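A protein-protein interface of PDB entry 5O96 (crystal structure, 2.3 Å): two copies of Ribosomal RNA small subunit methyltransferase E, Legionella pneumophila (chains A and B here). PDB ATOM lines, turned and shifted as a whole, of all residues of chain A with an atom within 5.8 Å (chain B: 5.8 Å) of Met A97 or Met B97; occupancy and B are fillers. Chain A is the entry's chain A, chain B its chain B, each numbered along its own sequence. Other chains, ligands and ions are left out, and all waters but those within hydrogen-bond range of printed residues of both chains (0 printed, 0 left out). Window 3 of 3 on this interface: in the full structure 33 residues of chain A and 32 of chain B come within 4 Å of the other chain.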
ATOM      1  N   GLY A  92     -15.992  28.143  14.322  1.00  0.00           N
ATOM      2  CA  GLY A  92     -15.049  28.927  15.083  1.00  0.00           C
ATOM      3  C   GLY A  92     -14.579  28.397  16.432  1.00  0.00           C
ATOM      4  O   GLY A  92     -14.004  27.303  16.542  1.00  0.00           O
ATOM      5  N   GLU A  93     -14.827  29.197  17.471  1.00  0.00           N
ATOM      6  CA  GLU A  93     -14.113  29.053  18.732  1.00  0.00           C
ATOM      7  C   GLU A  93     -14.742  27.978  19.602  1.00  0.00           C
ATOM      8  O   GLU A  93     -14.035  27.310  20.354  1.00  0.00           O
ATOM      9  CB  GLU A  93     -14.065  30.408  19.453  1.00  0.00           C
ATOM     10  CG  GLU A  93     -13.593  31.628  18.586  1.00  0.00           C
ATOM     11  CD  GLU A  93     -14.533  32.021  17.390  1.00  0.00           C
ATOM     12  OE1 GLU A  93     -15.780  32.103  17.545  1.00  0.00           O
ATOM     13  OE2 GLU A  93     -14.000  32.250  16.279  1.00  0.00           O
ATOM     14  N   ARG A  94     -16.053  27.778  19.485  1.00  0.00           N
ATOM     15  CA  ARG A  94     -16.696  26.743  20.273  1.00  0.00           C
ATOM     16  C   ARG A  94     -16.155  25.363  19.932  1.00  0.00           C
ATOM     17  O   ARG A  94     -15.971  24.528  20.821  1.00  0.00           O
ATOM     18  CB  ARG A  94     -18.205  26.786  20.070  1.00  0.00           C
ATOM     19  CG  ARG A  94     -18.851  28.090  20.496  1.00  0.00           C
ATOM     20  CD  ARG A  94     -20.371  27.948  20.381  1.00  0.00           C
ATOM     21  NE  ARG A  94     -21.038  29.098  19.787  1.00  0.00           N
ATOM     22  CZ  ARG A  94     -21.599  29.106  18.584  1.00  0.00           C
ATOM     23  NH1 ARG A  94     -21.566  28.025  17.825  1.00  0.00           N
ATOM     24  NH2 ARG A  94     -22.191  30.205  18.144  1.00  0.00           N
ATOM     25  N   MET A  95     -15.901  25.097  18.654  1.00  0.00           N
ATOM     26  CA  MET A  95     -15.370  23.792  18.285  1.00  0.00           C
ATOM     27  C   MET A  95     -13.962  23.598  18.843  1.00  0.00           C
ATOM     28  O   MET A  95     -13.618  22.508  19.316  1.00  0.00           O
ATOM     29  CB  MET A  95     -15.403  23.640  16.762  1.00  0.00           C
ATOM     30  CG  MET A  95     -15.360  22.193  16.219  1.00  0.00           C
ATOM     31  SD  MET A  95     -16.677  20.996  16.592  1.00  0.00           S
ATOM     32  CE  MET A  95     -18.033  21.952  17.194  1.00  0.00           C
ATOM     33  N   GLU A  96     -13.145  24.652  18.810  1.00  0.00           N
ATOM     34  CA  GLU A  96     -11.816  24.582  19.402  1.00  0.00           C
ATOM     35  C   GLU A  96     -11.904  24.353  20.901  1.00  0.00           C
ATOM     36  O   GLU A  96     -11.069  23.646  21.485  1.00  0.00           O
ATOM     37  CB  GLU A  96     -11.045  25.869  19.099  1.00  0.00           C
ATOM     38  CG  GLU A  96     -10.849  26.131  17.619  1.00  0.00           C
ATOM     39  CD  GLU A  96     -10.048  27.390  17.345  1.00  0.00           C
ATOM     40  OE1 GLU A  96     -10.059  28.287  18.205  1.00  0.00           O
ATOM     41  OE2 GLU A  96      -9.407  27.479  16.271  1.00  0.00           O
ATOM     42  N   MET A  97     -12.899  24.964  21.538  1.00  0.00           N
ATOM     43  CA  MET A  97     -13.128  24.735  22.950  1.00  0.00           C
ATOM     44  C   MET A  97     -13.382  23.256  23.219  1.00  0.00           C
ATOM     45  O   MET A  97     -12.766  22.660  24.118  1.00  0.00           O
ATOM     46  CB  MET A  97     -14.291  25.605  23.413  1.00  0.00           C
ATOM     47  CG  MET A  97     -14.561  25.614  24.940  1.00  0.00           C
ATOM     48  SD  MET A  97     -15.514  24.178  25.419  1.00  0.00           S
ATOM     49  CE  MET A  97     -16.579  24.951  26.643  1.00  0.00           C
ATOM     50  N   VAL A  98     -14.270  22.644  22.424  1.00  0.00           N
ATOM     51  CA  VAL A  98     -14.564  21.222  22.574  1.00  0.00           C
ATOM     52  C   VAL A  98     -13.316  20.386  22.333  1.00  0.00           C
ATOM     53  O   VAL A  98     -13.047  19.424  23.068  1.00  0.00           O
ATOM     54  CB  VAL A  98     -15.701  20.806  21.626  1.00  0.00           C
ATOM     55  CG1 VAL A  98     -15.912  19.281  21.664  1.00  0.00           C
ATOM     56  CG2 VAL A  98     -16.992  21.542  21.984  1.00  0.00           C
ATOM     57  N   MET A  99     -12.532  20.729  21.301  1.00  0.00           N
ATOM     58  CA  MET A  99     -11.314  19.964  21.046  1.00  0.00           C
ATOM     59  C   MET A  99     -10.391  19.971  22.261  1.00  0.00           C
ATOM     60  O   MET A  99      -9.846  18.930  22.651  1.00  0.00           O
ATOM     61  CB  MET A  99     -10.597  20.510  19.819  1.00  0.00           C
ATOM     62  CG  MET A  99     -11.393  20.365  18.517  1.00  0.00           C
ATOM     63  SD  MET A  99     -11.624  18.634  17.970  1.00  0.00           S
ATOM     64  CE  MET A  99     -13.331  18.665  17.503  1.00  0.00           C
ATOM     65  N   GLN A 100     -10.217  21.135  22.882  1.00  0.00           N
ATOM     66  CA  GLN A 100      -9.261  21.262  23.979  1.00  0.00           C
ATOM     67  C   GLN A 100      -9.727  20.506  25.223  1.00  0.00           C
ATOM     68  O   GLN A 100      -8.961  19.743  25.828  1.00  0.00           O
ATOM     69  CB  GLN A 100      -9.048  22.746  24.288  1.00  0.00           C
ATOM     70  CG  GLN A 100      -8.119  23.036  25.441  1.00  0.00           C
ATOM     71  CD  GLN A 100      -8.164  24.504  25.851  1.00  0.00           C
ATOM     72  OE1 GLN A 100      -9.076  24.938  26.541  1.00  0.00           O
ATOM     73  NE2 GLN A 100      -7.168  25.267  25.430  1.00  0.00           N
ATOM     74  N   LYS A 101     -10.983  20.680  25.592  1.00  0.00           N
ATOM     75  CA  LYS A 101     -11.499  20.222  26.869  1.00  0.00           C
ATOM     76  C   LYS A 101     -11.939  18.772  26.845  1.00  0.00           C
ATOM     77  O   LYS A 101     -11.881  18.094  27.871  1.00  0.00           O
ATOM     78  CB  LYS A 101     -12.648  21.136  27.290  1.00  0.00           C
ATOM     79  CG  LYS A 101     -12.173  22.573  27.444  1.00  0.00           C
ATOM     80  CD  LYS A 101     -12.923  23.328  28.471  1.00  0.00           C
ATOM     81  CE  LYS A 101     -12.356  24.732  28.577  1.00  0.00           C
ATOM     82  NZ  LYS A 101     -10.879  24.690  28.755  1.00  0.00           N
ATOM     83  N   SER A 102     -12.335  18.272  25.689  1.00  0.00           N
ATOM     84  CA  SER A 102     -12.665  16.862  25.610  1.00  0.00           C
ATOM     85  C   SER A 102     -11.401  16.023  25.758  1.00  0.00           C
ATOM     86  O   SER A 102     -11.413  14.984  26.439  1.00  0.00           O
ATOM     87  CB  SER A 102     -13.444  16.544  24.307  1.00  0.00           C
ATOM     88  OG  SER A 102     -12.678  16.667  23.127  1.00  0.00           O
ATOM     89  N   GLU A 228     -21.094  23.372  23.110  1.00  0.00           N
ATOM     90  CA  GLU A 228     -19.772  23.097  23.657  1.00  0.00           C
ATOM     91  C   GLU A 228     -19.835  22.791  25.151  1.00  0.00           C
ATOM     92  O   GLU A 228     -19.038  21.979  25.645  1.00  0.00           O
ATOM     93  CB  GLU A 228     -18.828  24.264  23.381  1.00  0.00           C
ATOM     94  CG  GLU A 228     -19.007  25.459  24.258  1.00  0.00           C
ATOM     95  CD  GLU A 228     -20.138  26.365  23.833  1.00  0.00           C
ATOM     96  OE1 GLU A 228     -20.838  26.068  22.839  1.00  0.00           O
ATOM     97  OE2 GLU A 228     -20.320  27.393  24.512  1.00  0.00           O
ATOM     98  N   THR A 229     -20.769  23.402  25.889  1.00  0.00           N
ATOM     99  CA  THR A 229     -20.931  22.997  27.281  1.00  0.00           C
ATOM    100  C   THR A 229     -21.311  21.534  27.338  1.00  0.00           C
ATOM    101  O   THR A 229     -20.796  20.774  28.165  1.00  0.00           O
ATOM    102  CB  THR A 229     -22.019  23.817  27.982  1.00  0.00           C
ATOM    103  OG1 THR A 229     -21.844  25.227  27.756  1.00  0.00           O
ATOM    104  CG2 THR A 229     -21.992  23.552  29.467  1.00  0.00           C
ATOM    105  N   ILE A 232     -18.579  18.811  27.321  1.00  0.00           N
ATOM    106  CA  ILE A 232     -17.693  18.686  28.475  1.00  0.00           C
ATOM    107  C   ILE A 232     -18.444  18.149  29.668  1.00  0.00           C
ATOM    108  O   ILE A 232     -17.956  17.260  30.379  1.00  0.00           O
ATOM    109  CB  ILE A 232     -17.050  20.033  28.789  1.00  0.00           C
ATOM    110  CG1 ILE A 232     -16.445  20.574  27.518  1.00  0.00           C
ATOM    111  CG2 ILE A 232     -15.967  19.887  29.834  1.00  0.00           C
ATOM    112  CD1 ILE A 232     -15.911  21.871  27.782  1.00  0.00           C
ATOM    113  N   GLY B  92      -8.948  37.339  32.477  1.00  0.00           N
ATOM    114  CA  GLY B  92      -9.795  37.608  31.327  1.00  0.00           C
ATOM    115  C   GLY B  92     -10.841  36.591  30.908  1.00  0.00           C
ATOM    116  O   GLY B  92     -11.851  36.395  31.596  1.00  0.00           O
ATOM    117  N   GLU B  93     -10.640  35.965  29.748  1.00  0.00           N
ATOM    118  CA  GLU B  93     -11.721  35.168  29.190  1.00  0.00           C
ATOM    119  C   GLU B  93     -11.926  33.857  29.952  1.00  0.00           C
ATOM    120  O   GLU B  93     -13.002  33.260  29.843  1.00  0.00           O
ATOM    121  CB  GLU B  93     -11.471  34.887  27.705  1.00  0.00           C
ATOM    122  CG  GLU B  93     -11.746  36.065  26.764  1.00  0.00           C
ATOM    123  CD  GLU B  93     -12.124  35.613  25.341  1.00  0.00           C
ATOM    124  OE1 GLU B  93     -12.941  36.299  24.683  1.00  0.00           O
ATOM    125  OE2 GLU B  93     -11.612  34.561  24.887  1.00  0.00           O
ATOM    126  N   ARG B  94     -10.936  33.393  30.724  1.00  0.00           N
ATOM    127  CA  ARG B  94     -11.142  32.182  31.518  1.00  0.00           C
ATOM    128  C   ARG B  94     -12.241  32.396  32.554  1.00  0.00           C
ATOM    129  O   ARG B  94     -13.137  31.554  32.713  1.00  0.00           O
ATOM    130  CB  ARG B  94      -9.839  31.754  32.187  1.00  0.00           C
ATOM    131  CG  ARG B  94      -8.695  31.512  31.220  1.00  0.00           C
ATOM    132  CD  ARG B  94      -7.414  31.268  31.991  1.00  0.00           C
ATOM    133  NE  ARG B  94      -6.267  31.996  31.455  1.00  0.00           N
ATOM    134  CZ  ARG B  94      -5.177  31.412  30.978  1.00  0.00           C
ATOM    135  NH1 ARG B  94      -4.164  32.145  30.517  1.00  0.00           N
ATOM    136  NH2 ARG B  94      -5.098  30.090  30.974  1.00  0.00           N
ATOM    137  N   MET B  95     -12.204  33.535  33.252  1.00  0.00           N
ATOM    138  CA  MET B  95     -13.201  33.784  34.284  1.00  0.00           C
ATOM    139  C   MET B  95     -14.582  33.999  33.678  1.00  0.00           C
ATOM    140  O   MET B  95     -15.593  33.588  34.264  1.00  0.00           O
ATOM    141  CB  MET B  95     -12.784  34.987  35.123  1.00  0.00           C
ATOM    142  CG  MET B  95     -13.373  34.966  36.502  1.00  0.00           C
ATOM    143  SD  MET B  95     -12.772  33.557  37.483  1.00  0.00           S
ATOM    144  CE  MET B  95     -13.620  33.940  39.028  1.00  0.00           C
ATOM    145  N   GLU B  96     -14.641  34.634  32.508  1.00  0.00           N
ATOM    146  CA  GLU B  96     -15.899  34.756  31.784  1.00  0.00           C
ATOM    147  C   GLU B  96     -16.489  33.389  31.477  1.00  0.00           C
ATOM    148  O   GLU B  96     -17.704  33.202  31.576  1.00  0.00           O
ATOM    149  CB  GLU B  96     -15.701  35.553  30.489  1.00  0.00           C
ATOM    150  CG  GLU B  96     -15.305  37.017  30.711  1.00  0.00           C
ATOM    151  CD  GLU B  96     -15.025  37.749  29.407  1.00  0.00           C
ATOM    152  OE1 GLU B  96     -14.942  37.097  28.343  1.00  0.00           O
ATOM    153  OE2 GLU B  96     -14.887  38.982  29.445  1.00  0.00           O
ATOM    154  N   MET B  97     -15.651  32.415  31.108  1.00  0.00           N
ATOM    155  CA  MET B  97     -16.202  31.093  30.834  1.00  0.00           C
ATOM    156  C   MET B  97     -16.815  30.475  32.093  1.00  0.00           C
ATOM    157  O   MET B  97     -17.932  29.928  32.045  1.00  0.00           O
ATOM    158  CB  MET B  97     -15.153  30.161  30.234  1.00  0.00           C
ATOM    159  CG  MET B  97     -15.845  28.886  29.767  1.00  0.00           C
ATOM    160  SD  MET B  97     -14.826  27.721  28.899  1.00  0.00           S
ATOM    161  CE  MET B  97     -14.401  28.657  27.415  1.00  0.00           C
ATOM    162  N   VAL B  98     -16.116  30.583  33.234  1.00  0.00           N
ATOM    163  CA  VAL B  98     -16.639  30.072  34.506  1.00  0.00           C
ATOM    164  C   VAL B  98     -18.004  30.673  34.811  1.00  0.00           C
ATOM    165  O   VAL B  98     -18.952  29.950  35.131  1.00  0.00           O
ATOM    166  CB  VAL B  98     -15.653  30.346  35.661  1.00  0.00           C
ATOM    167  CG1 VAL B  98     -16.218  29.834  36.961  1.00  0.00           C
ATOM    168  CG2 VAL B  98     -14.320  29.698  35.413  1.00  0.00           C
ATOM    169  N   MET B  99     -18.124  32.011  34.738  1.00  0.00           N
ATOM    170  CA  MET B  99     -19.414  32.655  35.009  1.00  0.00           C
ATOM    171  C   MET B  99     -20.516  32.094  34.111  1.00  0.00           C
ATOM    172  O   MET B  99     -21.596  31.751  34.590  1.00  0.00           O
ATOM    173  CB  MET B  99     -19.300  34.181  34.855  1.00  0.00           C
ATOM    174  CG  MET B  99     -18.350  34.859  35.889  1.00  0.00           C
ATOM    175  SD  MET B  99     -18.939  34.752  37.572  1.00  0.00           S
ATOM    176  CE  MET B  99     -17.465  35.226  38.467  1.00  0.00           C
ATOM    177  N   GLN B 100     -20.249  31.952  32.815  1.00  0.00           N
ATOM    178  CA  GLN B 100     -21.282  31.445  31.913  1.00  0.00           C
ATOM    179  C   GLN B 100     -21.599  29.976  32.189  1.00  0.00           C
ATOM    180  O   GLN B 100     -22.763  29.618  32.412  1.00  0.00           O
ATOM    181  CB  GLN B 100     -20.863  31.617  30.453  1.00  0.00           C
ATOM    182  CG  GLN B 100     -21.917  31.147  29.452  1.00  0.00           C
ATOM    183  CD  GLN B 100     -21.399  31.141  28.034  1.00  0.00           C
ATOM    184  OE1 GLN B 100     -20.532  30.357  27.683  1.00  0.00           O
ATOM    185  NE2 GLN B 100     -21.929  32.020  27.213  1.00  0.00           N
ATOM    186  N   LYS B 101     -20.578  29.108  32.159  1.00  0.00           N
ATOM    187  CA  LYS B 101     -20.837  27.675  32.280  1.00  0.00           C
ATOM    188  C   LYS B 101     -21.449  27.339  33.625  1.00  0.00           C
ATOM    189  O   LYS B 101     -22.345  26.489  33.718  1.00  0.00           O
ATOM    190  CB  LYS B 101     -19.558  26.858  32.088  1.00  0.00           C
ATOM    191  CG  LYS B 101     -18.919  26.947  30.729  1.00  0.00           C
ATOM    192  CD  LYS B 101     -19.921  26.933  29.628  1.00  0.00           C
ATOM    193  CE  LYS B 101     -19.228  27.095  28.300  1.00  0.00           C
ATOM    194  NZ  LYS B 101     -20.195  27.380  27.205  1.00  0.00           N
ATOM    195  N   SER B 102     -20.984  27.994  34.688  1.00  0.00           N
ATOM    196  CA  SER B 102     -21.503  27.641  35.996  1.00  0.00           C
ATOM    197  C   SER B 102     -22.975  28.016  36.118  1.00  0.00           C
ATOM    198  O   SER B 102     -23.744  27.310  36.783  1.00  0.00           O
ATOM    199  CB  SER B 102     -20.646  28.299  37.092  1.00  0.00           C
ATOM    200  OG  SER B 102     -20.874  29.691  37.166  1.00  0.00           O
ATOM    201  N   GLU B 228     -10.788  26.718  34.458  1.00  0.00           N
ATOM    202  CA  GLU B 228     -12.169  26.876  34.036  1.00  0.00           C
ATOM    203  C   GLU B 228     -12.798  25.534  33.626  1.00  0.00           C
ATOM    204  O   GLU B 228     -14.004  25.332  33.842  1.00  0.00           O
ATOM    205  CB  GLU B 228     -12.236  27.927  32.918  1.00  0.00           C
ATOM    206  CG  GLU B 228     -11.848  27.435  31.519  1.00  0.00           C
ATOM    207  CD  GLU B 228     -10.339  27.488  31.233  1.00  0.00           C
ATOM    208  OE1 GLU B 228      -9.575  27.913  32.123  1.00  0.00           O
ATOM    209  OE2 GLU B 228      -9.911  27.107  30.116  1.00  0.00           O
ATOM    210  N   ILE B 232     -16.332  23.557  35.229  1.00  0.00           N
ATOM    211  CA  ILE B 232     -17.368  22.868  34.450  1.00  0.00           C
ATOM    212  C   ILE B 232     -17.513  21.427  34.914  1.00  0.00           C
ATOM    213  O   ILE B 232     -18.618  20.949  35.193  1.00  0.00           O
ATOM    214  CB  ILE B 232     -17.060  22.911  32.946  1.00  0.00           C
ATOM    215  CG1 ILE B 232     -16.999  24.348  32.427  1.00  0.00           C
ATOM    216  CG2 ILE B 232     -18.116  22.131  32.193  1.00  0.00           C
ATOM    217  CD1 ILE B 232     -16.387  24.440  31.010  1.00  0.00           C
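The side-chain amino group (NZ) of Lys A101 is in salt-bridge range of the side-chain carboxylate (OE2) of Glu B228 (2.9 Å). OE2 of Glu A228 lies within salt-bridge range of NZ of Lys B101 (2.7 Å). OG1 of Thr A229 sits at hydrogen-bond distance from NZ of Lys B101 (2.8 Å).
The side-chain amide oxygen of Gln A100 lies within hydrogen-bond range of the side-chain amino group of Lys A101, at 2.9 Å. The side-chain amino group (NZ) of Lys B101 sits at hydrogen-bond distance from the side-chain amide oxygen (OE1) of Gln B100.
Among the printed residues, pairs that only touch across the chains: Met A97 with Met B97, Met A97 with Lys B101, Lys A101 with Met B97 and Ile A232 with Ile B232.
Of chain B, only Met B97 (3.9 Å) and Lys B101 (3.8 Å) come within 4 Å of Met A97. Met B97 touches just these residues of chain A: Met A97 (3.9 Å) and Lys A101 (3.9 Å). Printed residues of chain B within 4 Å of Thr A229: Lys B101. Of the printed residues of chain A, Lys B101 touches Met A97 (3.8 Å), Glu A228 (2.7 Å) and Thr A229 (2.8 Å). Of the printed residues of chain B, Glu A228 touches Lys B101. Met B95 touches none of the printed residues of chain A. Glu B96 touches none of the printed residues of chain A. The nearest printed residue of chain A that does not touch Ile B232 is Met A97 (4.4 Å).
Of the 13 printed residues of chain B, 4 touch a printed residue of chain A. Hydrophobic or aromatic side chains of chain A that line the printed part of chain B: Met A97 and Ile A232. Along chain A the printed residues that touch a printed residue of chain B span positions 97 to 232.
Met B97 touches its own counterpart, Met A97. Met A97 touches Lys B101, and with the chains exchanged Lys A101 touches Met B97. Lys A101 touches Glu B228, and with the chains exchanged Glu A228 touches Lys B101. Ile A232 touches its own counterpart, Ile B232.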
